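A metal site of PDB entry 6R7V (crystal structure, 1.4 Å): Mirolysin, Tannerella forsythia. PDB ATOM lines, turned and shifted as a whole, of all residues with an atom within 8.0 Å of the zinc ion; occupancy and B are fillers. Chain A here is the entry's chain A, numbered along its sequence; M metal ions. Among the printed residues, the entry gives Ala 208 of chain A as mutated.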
ATOM      1  N   ARG A   4      22.078 -16.456  -3.176  1.00  0.00           N
ATOM      2  CA  ARG A   4      23.133 -17.471  -3.174  1.00  0.00           C
ATOM      3  C   ARG A   4      22.717 -18.682  -4.025  1.00  0.00           C
ATOM      4  O   ARG A   4      21.533 -19.041  -4.045  1.00  0.00           O
ATOM      5  CB  ARG A   4      23.456 -17.868  -1.716  1.00  0.00           C
ATOM      6  CG  ARG A   4      24.306 -19.113  -1.498  1.00  0.00           C
ATOM      7  CD  ARG A   4      24.580 -19.401  -0.004  1.00  0.00           C
ATOM      8  NE  ARG A   4      25.035 -18.230   0.758  1.00  0.00           N
ATOM      9  CZ  ARG A   4      26.258 -17.704   0.677  1.00  0.00           C
ATOM     10  NH1 ARG A   4      27.167 -18.209  -0.151  1.00  0.00           N
ATOM     11  NH2 ARG A   4      26.578 -16.651   1.426  1.00  0.00           N
ATOM     12  N   THR A   5      23.672 -19.284  -4.771  1.00  0.00           N
ATOM     13  CA  THR A   5      23.438 -20.487  -5.570  1.00  0.00           C
ATOM     14  C   THR A   5      24.258 -21.611  -4.965  1.00  0.00           C
ATOM     15  O   THR A   5      25.381 -21.375  -4.499  1.00  0.00           O
ATOM     16  CB  THR A   5      23.756 -20.280  -7.036  1.00  0.00           C
ATOM     17  OG1 THR A   5      25.100 -19.835  -7.097  1.00  0.00           O
ATOM     18  CG2 THR A   5      22.813 -19.303  -7.713  1.00  0.00           C
ATOM     19  N   CYS A   6      23.708 -22.811  -4.927  1.00  0.00           N
ATOM     20  CA  CYS A   6      24.344 -23.954  -4.312  1.00  0.00           C
ATOM     21  C   CYS A   6      23.924 -25.213  -4.988  1.00  0.00           C
ATOM     22  O   CYS A   6      22.729 -25.366  -5.289  1.00  0.00           O
ATOM     23  CB  CYS A   6      24.008 -23.972  -2.823  1.00  0.00           C
ATOM     24  SG  CYS A   6      24.673 -25.391  -1.918  1.00  0.00           S
ATOM     25  N   GLY A   7      24.858 -26.124  -5.224  1.00  0.00           N
ATOM     26  CA  GLY A   7      24.507 -27.383  -5.878  1.00  0.00           C
ATOM     27  C   GLY A   7      24.179 -28.497  -4.903  1.00  0.00           C
ATOM     28  O   GLY A   7      24.124 -29.669  -5.333  1.00  0.00           O
ATOM     29  N   SER A   8      23.947 -28.186  -3.601  1.00  0.00           N
ATOM     30  CA  SER A   8      23.667 -29.229  -2.623  1.00  0.00           C
ATOM     31  C   SER A   8      22.296 -29.129  -1.979  1.00  0.00           C
ATOM     32  O   SER A   8      22.148 -29.281  -0.778  1.00  0.00           O
ATOM     33  CB  SER A   8      24.738 -29.222  -1.535  1.00  0.00           C
ATOM     34  OG  SER A   8      26.013 -29.497  -2.104  1.00  0.00           O
ATOM     35  N   GLU A   9      21.277 -28.969  -2.805  1.00  0.00           N
ATOM     36  CA  GLU A   9      19.905 -28.999  -2.320  1.00  0.00           C
ATOM     37  C   GLU A   9      19.455 -30.453  -2.179  1.00  0.00           C
ATOM     38  O   GLU A   9      19.829 -31.283  -2.995  1.00  0.00           O
ATOM     39  CB  GLU A   9      18.979 -28.233  -3.283  1.00  0.00           C
ATOM     40  CG  GLU A   9      19.260 -26.725  -3.328  1.00  0.00           C
ATOM     41  CD  GLU A   9      18.493 -25.869  -4.330  1.00  0.00           C
ATOM     42  OE1 GLU A   9      18.706 -24.640  -4.328  1.00  0.00           O
ATOM     43  OE2 GLU A   9      17.693 -26.426  -5.110  1.00  0.00           O
ATOM     44  N   LEU A  10      18.601 -30.735  -1.190  1.00  0.00           N
ATOM     45  CA  LEU A  10      18.017 -32.049  -0.985  1.00  0.00           C
ATOM     46  C   LEU A  10      16.512 -31.932  -0.897  1.00  0.00           C
ATOM     47  O   LEU A  10      15.940 -31.938   0.203  1.00  0.00           O
ATOM     48  CB  LEU A  10      18.572 -32.769   0.259  1.00  0.00           C
ATOM     49  CG  LEU A  10      20.064 -33.184   0.210  1.00  0.00           C
ATOM     50  CD1 LEU A  10      20.491 -33.771   1.567  1.00  0.00           C
ATOM     51  CD2 LEU A  10      20.335 -34.227  -0.901  1.00  0.00           C
ATOM     52  N   GLY A 165      29.043 -22.722  -5.308  1.00  0.00           N
ATOM     53  CA  GLY A 165      29.752 -23.837  -4.711  1.00  0.00           C
ATOM     54  C   GLY A 165      28.854 -25.043  -4.550  1.00  0.00           C
ATOM     55  O   GLY A 165      27.619 -24.934  -4.731  1.00  0.00           O
ATOM     56  N   TYR A 166      29.454 -26.189  -4.229  1.00  0.00           N
ATOM     57  CA  TYR A 166      28.687 -27.399  -3.939  1.00  0.00           C
ATOM     58  C   TYR A 166      29.522 -28.343  -3.081  1.00  0.00           C
ATOM     59  O   TYR A 166      30.751 -28.290  -3.093  1.00  0.00           O
ATOM     60  CB  TYR A 166      28.170 -28.082  -5.202  1.00  0.00           C
ATOM     61  CG  TYR A 166      29.203 -28.728  -6.091  1.00  0.00           C
ATOM     62  CD1 TYR A 166      29.476 -30.101  -5.997  1.00  0.00           C
ATOM     63  CD2 TYR A 166      29.838 -28.002  -7.099  1.00  0.00           C
ATOM     64  CE1 TYR A 166      30.394 -30.714  -6.849  1.00  0.00           C
ATOM     65  CE2 TYR A 166      30.731 -28.618  -7.964  1.00  0.00           C
ATOM     66  CZ  TYR A 166      30.985 -29.976  -7.854  1.00  0.00           C
ATOM     67  OH  TYR A 166      31.891 -30.582  -8.701  1.00  0.00           O
ATOM     68  N   ALA A 167      28.846 -29.211  -2.347  1.00  0.00           N
ATOM     69  CA  ALA A 167      29.497 -30.173  -1.478  1.00  0.00           C
ATOM     70  C   ALA A 167      28.964 -31.542  -1.723  1.00  0.00           C
ATOM     71  O   ALA A 167      27.815 -31.685  -2.162  1.00  0.00           O
ATOM     72  CB  ALA A 167      29.232 -29.779  -0.023  1.00  0.00           C
ATOM     73  N   PHE A 169      27.628 -34.838   0.327  1.00  0.00           N
ATOM     74  CA  PHE A 169      27.156 -35.161   1.670  1.00  0.00           C
ATOM     75  C   PHE A 169      27.767 -36.453   2.216  1.00  0.00           C
ATOM     76  O   PHE A 169      28.071 -37.363   1.423  1.00  0.00           O
ATOM     77  CB  PHE A 169      25.626 -35.330   1.645  1.00  0.00           C
ATOM     78  CG  PHE A 169      24.858 -34.047   1.490  1.00  0.00           C
ATOM     79  CD1 PHE A 169      24.336 -33.673   0.255  1.00  0.00           C
ATOM     80  CD2 PHE A 169      24.651 -33.213   2.572  1.00  0.00           C
ATOM     81  CE1 PHE A 169      23.679 -32.452   0.104  1.00  0.00           C
ATOM     82  CE2 PHE A 169      23.940 -32.015   2.434  1.00  0.00           C
ATOM     83  CZ  PHE A 169      23.441 -31.647   1.203  1.00  0.00           C
ATOM     84  N   THR A 204      30.682 -18.707   1.572  1.00  0.00           N
ATOM     85  CA  THR A 204      30.305 -19.750   0.621  1.00  0.00           C
ATOM     86  C   THR A 204      30.953 -21.064   1.091  1.00  0.00           C
ATOM     87  O   THR A 204      30.307 -22.119   1.139  1.00  0.00           O
ATOM     88  CB  THR A 204      30.686 -19.380  -0.817  1.00  0.00           C
ATOM     89  OG1 THR A 204      30.013 -18.164  -1.153  1.00  0.00           O
ATOM     90  CG2 THR A 204      30.294 -20.451  -1.808  1.00  0.00           C
ATOM     91  N   HIS A 207      29.320 -22.386   4.399  1.00  0.00           N
ATOM     92  CA  HIS A 207      28.057 -23.041   4.060  1.00  0.00           C
ATOM     93  C   HIS A 207      28.324 -24.440   3.440  1.00  0.00           C
ATOM     94  O   HIS A 207      27.682 -25.424   3.840  1.00  0.00           O
ATOM     95  CB  HIS A 207      27.340 -22.115   3.071  1.00  0.00           C
ATOM     96  CG  HIS A 207      26.083 -22.638   2.481  1.00  0.00           C
ATOM     97  ND1 HIS A 207      24.842 -22.165   2.881  1.00  0.00           N
ATOM     98  CD2 HIS A 207      25.906 -23.552   1.484  1.00  0.00           C
ATOM     99  CE1 HIS A 207      23.969 -22.800   2.115  1.00  0.00           C
ATOM    100  NE2 HIS A 207      24.567 -23.655   1.282  1.00  0.00           N
ATOM    101  N   ALA A 208      29.266 -24.535   2.474  1.00  0.00           N
ATOM    102  CA  ALA A 208      29.554 -25.808   1.808  1.00  0.00           C
ATOM    103  C   ALA A 208      30.123 -26.803   2.781  1.00  0.00           C
ATOM    104  O   ALA A 208      29.776 -27.988   2.719  1.00  0.00           O
ATOM    105  CB  ALA A 208      30.535 -25.601   0.669  1.00  0.00           C
ATOM    106  N   GLY A 210      29.532 -26.886   5.899  1.00  0.00           N
ATOM    107  CA  GLY A 210      28.380 -27.320   6.679  1.00  0.00           C
ATOM    108  C   GLY A 210      27.712 -28.516   6.009  1.00  0.00           C
ATOM    109  O   GLY A 210      27.407 -29.495   6.676  1.00  0.00           O
ATOM    110  N   HIS A 211      27.473 -28.470   4.660  1.00  0.00           N
ATOM    111  CA  HIS A 211      26.919 -29.673   3.976  1.00  0.00           C
ATOM    112  C   HIS A 211      27.842 -30.892   4.050  1.00  0.00           C
ATOM    113  O   HIS A 211      27.365 -32.016   4.230  1.00  0.00           O
ATOM    114  CB  HIS A 211      26.670 -29.382   2.497  1.00  0.00           C
ATOM    115  CG  HIS A 211      25.611 -28.350   2.184  1.00  0.00           C
ATOM    116  ND1 HIS A 211      24.307 -28.476   2.640  1.00  0.00           N
ATOM    117  CD2 HIS A 211      25.681 -27.299   1.342  1.00  0.00           C
ATOM    118  CE1 HIS A 211      23.623 -27.483   2.067  1.00  0.00           C
ATOM    119  NE2 HIS A 211      24.394 -26.772   1.268  1.00  0.00           N
ATOM    120  N   LEU A 215      24.956 -30.970   7.227  1.00  0.00           N
ATOM    121  CA  LEU A 215      23.861 -30.016   7.378  1.00  0.00           C
ATOM    122  C   LEU A 215      23.125 -29.799   6.077  1.00  0.00           C
ATOM    123  O   LEU A 215      23.746 -29.815   4.981  1.00  0.00           O
ATOM    124  CB  LEU A 215      24.368 -28.660   7.870  1.00  0.00           C
ATOM    125  CG  LEU A 215      25.113 -28.663   9.199  1.00  0.00           C
ATOM    126  CD1 LEU A 215      25.439 -27.250   9.625  1.00  0.00           C
ATOM    127  CD2 LEU A 215      24.312 -29.395  10.298  1.00  0.00           C
ATOM    128  N   ARG A 216      21.846 -29.477   6.201  1.00  0.00           N
ATOM    129  CA  ARG A 216      20.975 -29.169   5.074  1.00  0.00           C
ATOM    130  C   ARG A 216      20.583 -27.713   5.086  1.00  0.00           C
ATOM    131  O   ARG A 216      20.567 -27.042   6.138  1.00  0.00           O
ATOM    132  CB  ARG A 216      19.691 -29.989   5.176  1.00  0.00           C
ATOM    133  CG  ARG A 216      19.936 -31.471   5.068  1.00  0.00           C
ATOM    134  CD  ARG A 216      18.627 -32.164   4.917  1.00  0.00           C
ATOM    135  NE  ARG A 216      18.770 -33.602   5.063  1.00  0.00           N
ATOM    136  CZ  ARG A 216      17.782 -34.468   4.843  1.00  0.00           C
ATOM    137  NH1 ARG A 216      16.610 -34.038   4.402  1.00  0.00           N
ATOM    138  NH2 ARG A 216      17.972 -35.762   5.052  1.00  0.00           N
ATOM    139  N   HIS A 217      20.095 -27.243   3.945  1.00  0.00           N
ATOM    140  CA  HIS A 217      19.517 -25.904   3.876  1.00  0.00           C
ATOM    141  C   HIS A 217      18.443 -25.736   4.930  1.00  0.00           C
ATOM    142  O   HIS A 217      17.599 -26.623   5.105  1.00  0.00           O
ATOM    143  CB  HIS A 217      18.939 -25.666   2.509  1.00  0.00           C
ATOM    144  CG  HIS A 217      19.999 -25.531   1.477  1.00  0.00           C
ATOM    145  ND1 HIS A 217      19.790 -25.933   0.192  1.00  0.00           N
ATOM    146  CD2 HIS A 217      21.261 -25.070   1.599  1.00  0.00           C
ATOM    147  CE1 HIS A 217      20.913 -25.679  -0.461  1.00  0.00           C
ATOM    148  NE2 HIS A 217      21.847 -25.203   0.346  1.00  0.00           N
ATOM    149  N   ILE A 218      18.480 -24.596   5.614  1.00  0.00           N
ATOM    150  CA  ILE A 218      17.643 -24.379   6.802  1.00  0.00           C
ATOM    151  C   ILE A 218      16.133 -24.405   6.470  1.00  0.00           C
ATOM    152  O   ILE A 218      15.315 -24.781   7.313  1.00  0.00           O
ATOM    153  CB  ILE A 218      18.059 -23.058   7.474  1.00  0.00           C
ATOM    154  CG1 ILE A 218      17.375 -22.889   8.833  1.00  0.00           C
ATOM    155  CG2 ILE A 218      17.809 -21.832   6.554  1.00  0.00           C
ATOM    156  CD1 ILE A 218      18.042 -21.815   9.701  1.00  0.00           C
ATOM    157  N   TRP A 219      15.762 -24.032   5.243  1.00  0.00           N
ATOM    158  CA  TRP A 219      14.346 -24.011   4.866  1.00  0.00           C
ATOM    159  C   TRP A 219      13.818 -25.372   4.370  1.00  0.00           C
ATOM    160  O   TRP A 219      12.617 -25.480   4.043  1.00  0.00           O
ATOM    161  CB  TRP A 219      14.065 -22.918   3.828  1.00  0.00           C
ATOM    162  CG  TRP A 219      14.624 -23.218   2.483  1.00  0.00           C
ATOM    163  CD1 TRP A 219      13.983 -23.814   1.433  1.00  0.00           C
ATOM    164  CD2 TRP A 219      15.973 -22.984   2.056  1.00  0.00           C
ATOM    165  NE1 TRP A 219      14.864 -23.971   0.384  1.00  0.00           N
ATOM    166  CE2 TRP A 219      16.078 -23.460   0.724  1.00  0.00           C
ATOM    167  CE3 TRP A 219      17.085 -22.355   2.636  1.00  0.00           C
ATOM    168  CZ2 TRP A 219      17.272 -23.365  -0.006  1.00  0.00           C
ATOM    169  CZ3 TRP A 219      18.262 -22.275   1.909  1.00  0.00           C
ATOM    170  CH2 TRP A 219      18.339 -22.757   0.585  1.00  0.00           C
ATOM    171  N   ASP A 221      14.578 -27.254   1.570  1.00  0.00           N
ATOM    172  CA  ASP A 221      14.622 -27.508   0.131  1.00  0.00           C
ATOM    173  C   ASP A 221      13.272 -27.982  -0.364  1.00  0.00           C
ATOM    174  O   ASP A 221      13.173 -29.000  -1.049  1.00  0.00           O
ATOM    175  CB  ASP A 221      15.718 -28.575  -0.157  1.00  0.00           C
ATOM    176  CG  ASP A 221      17.113 -28.032   0.018  1.00  0.00           C
ATOM    177  OD1 ASP A 221      17.396 -26.963  -0.530  1.00  0.00           O
ATOM    178  OD2 ASP A 221      17.931 -28.688   0.719  1.00  0.00           O
ATOM    179  N   TYR A 266      24.271 -19.809   8.684  1.00  0.00           N
ATOM    180  CA  TYR A 266      25.100 -20.070   7.504  1.00  0.00           C
ATOM    181  C   TYR A 266      24.452 -20.969   6.469  1.00  0.00           C
ATOM    182  O   TYR A 266      24.873 -20.942   5.301  1.00  0.00           O
ATOM    183  CB  TYR A 266      26.425 -20.724   7.921  1.00  0.00           C
ATOM    184  CG  TYR A 266      27.257 -19.879   8.876  1.00  0.00           C
ATOM    185  CD1 TYR A 266      27.642 -18.586   8.550  1.00  0.00           C
ATOM    186  CD2 TYR A 266      27.617 -20.360  10.127  1.00  0.00           C
ATOM    187  CE1 TYR A 266      28.339 -17.779   9.447  1.00  0.00           C
ATOM    188  CE2 TYR A 266      28.351 -19.576  11.021  1.00  0.00           C
ATOM    189  CZ  TYR A 266      28.700 -18.287  10.674  1.00  0.00           C
ATOM    190  OH  TYR A 266      29.400 -17.509  11.557  1.00  0.00           O
ATOM    191  N   MET A 267      23.438 -21.758   6.850  1.00  0.00           N
ATOM    192  CA  MET A 267      22.801 -22.672   5.925  1.00  0.00           C
ATOM    193  C   MET A 267      21.596 -22.061   5.208  1.00  0.00           C
ATOM    194  O   MET A 267      20.826 -22.790   4.581  1.00  0.00           O
ATOM    195  CB  MET A 267      22.399 -23.968   6.654  1.00  0.00           C
ATOM    196  CG  MET A 267      23.619 -24.697   7.283  1.00  0.00           C
ATOM    197  SD  MET A 267      25.110 -24.833   6.224  1.00  0.00           S
ATOM    198  CE  MET A 267      24.465 -25.846   4.863  1.00  0.00           C
ATOM    199  N   ASP A 268      21.484 -20.727   5.241  1.00  0.00           N
ATOM    200  CA  ASP A 268      20.486 -20.037   4.418  1.00  0.00           C
ATOM    201  C   ASP A 268      21.215 -19.560   3.139  1.00  0.00           C
ATOM    202  O   ASP A 268      22.353 -19.991   2.867  1.00  0.00           O
ATOM    203  CB  ASP A 268      19.798 -18.881   5.190  1.00  0.00           C
ATOM    204  CG  ASP A 268      18.370 -18.578   4.708  1.00  0.00           C
ATOM    205  OD1 ASP A 268      18.086 -18.824   3.523  1.00  0.00           O
ATOM    206  OD2 ASP A 268      17.555 -18.134   5.514  1.00  0.00           O
ATOM    207  N   TYR A 269      20.561 -18.708   2.313  1.00  0.00           N
ATOM    208  CA  TYR A 269      21.119 -18.207   1.055  1.00  0.00           C
ATOM    209  C   TYR A 269      21.410 -16.713   1.111  1.00  0.00           C
ATOM    210  O   TYR A 269      21.557 -16.069   0.071  1.00  0.00           O
ATOM    211  CB  TYR A 269      20.173 -18.483  -0.127  1.00  0.00           C
ATOM    212  CG  TYR A 269      20.272 -19.847  -0.787  1.00  0.00           C
ATOM    213  CD1 TYR A 269      21.239 -20.765  -0.395  1.00  0.00           C
ATOM    214  CD2 TYR A 269      19.422 -20.197  -1.837  1.00  0.00           C
ATOM    215  CE1 TYR A 269      21.378 -21.987  -1.054  1.00  0.00           C
ATOM    216  CE2 TYR A 269      19.543 -21.415  -2.480  1.00  0.00           C
ATOM    217  CZ  TYR A 269      20.532 -22.305  -2.102  1.00  0.00           C
ATOM    218  OH  TYR A 269      20.612 -23.536  -2.713  1.00  0.00           O
HETATM  219 ZN    ZN M   1      23.866 -25.167   0.131  1.00  0.00          ZN
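O of Leu 215 sits at hydrogen-bond distance from ND1 of His 211 (2.8 Å).
A ring nitrogen (ND1) of His 207 lies within hydrogen-bond range of the backbone carbonyl oxygen of Tyr 266 (2.7 Å).
The backbone carbonyl oxygen (O) of Asp 268 lies within hydrogen-bond range of a ring nitrogen (ND1) of His 207 (3.3 Å).
The side-chain carboxylate (OD1) of Asp 221 is in hydrogen-bond range of a ring nitrogen (ND1) of His 217, 2.7 Å away.
N of Ser 8 lies close to SG of Cys 6.
The zinc ion is bound by a ring nitrogen (NE2) of His 207 (2.0 Å), a ring nitrogen (NE2) of His 217 (2.0 Å), a ring nitrogen (NE2) of His 211 (2.0 Å) and the side-chain sulfur of Cys 6 (2.2 Å).
The zinc ion has four donor atoms within binding distance.
Of the 26 residues printed, 4 come within 4 Å of the zinc ion.
The nearest printed residue that does not touch the zinc ion is Tyr 269 (4.2 Å).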
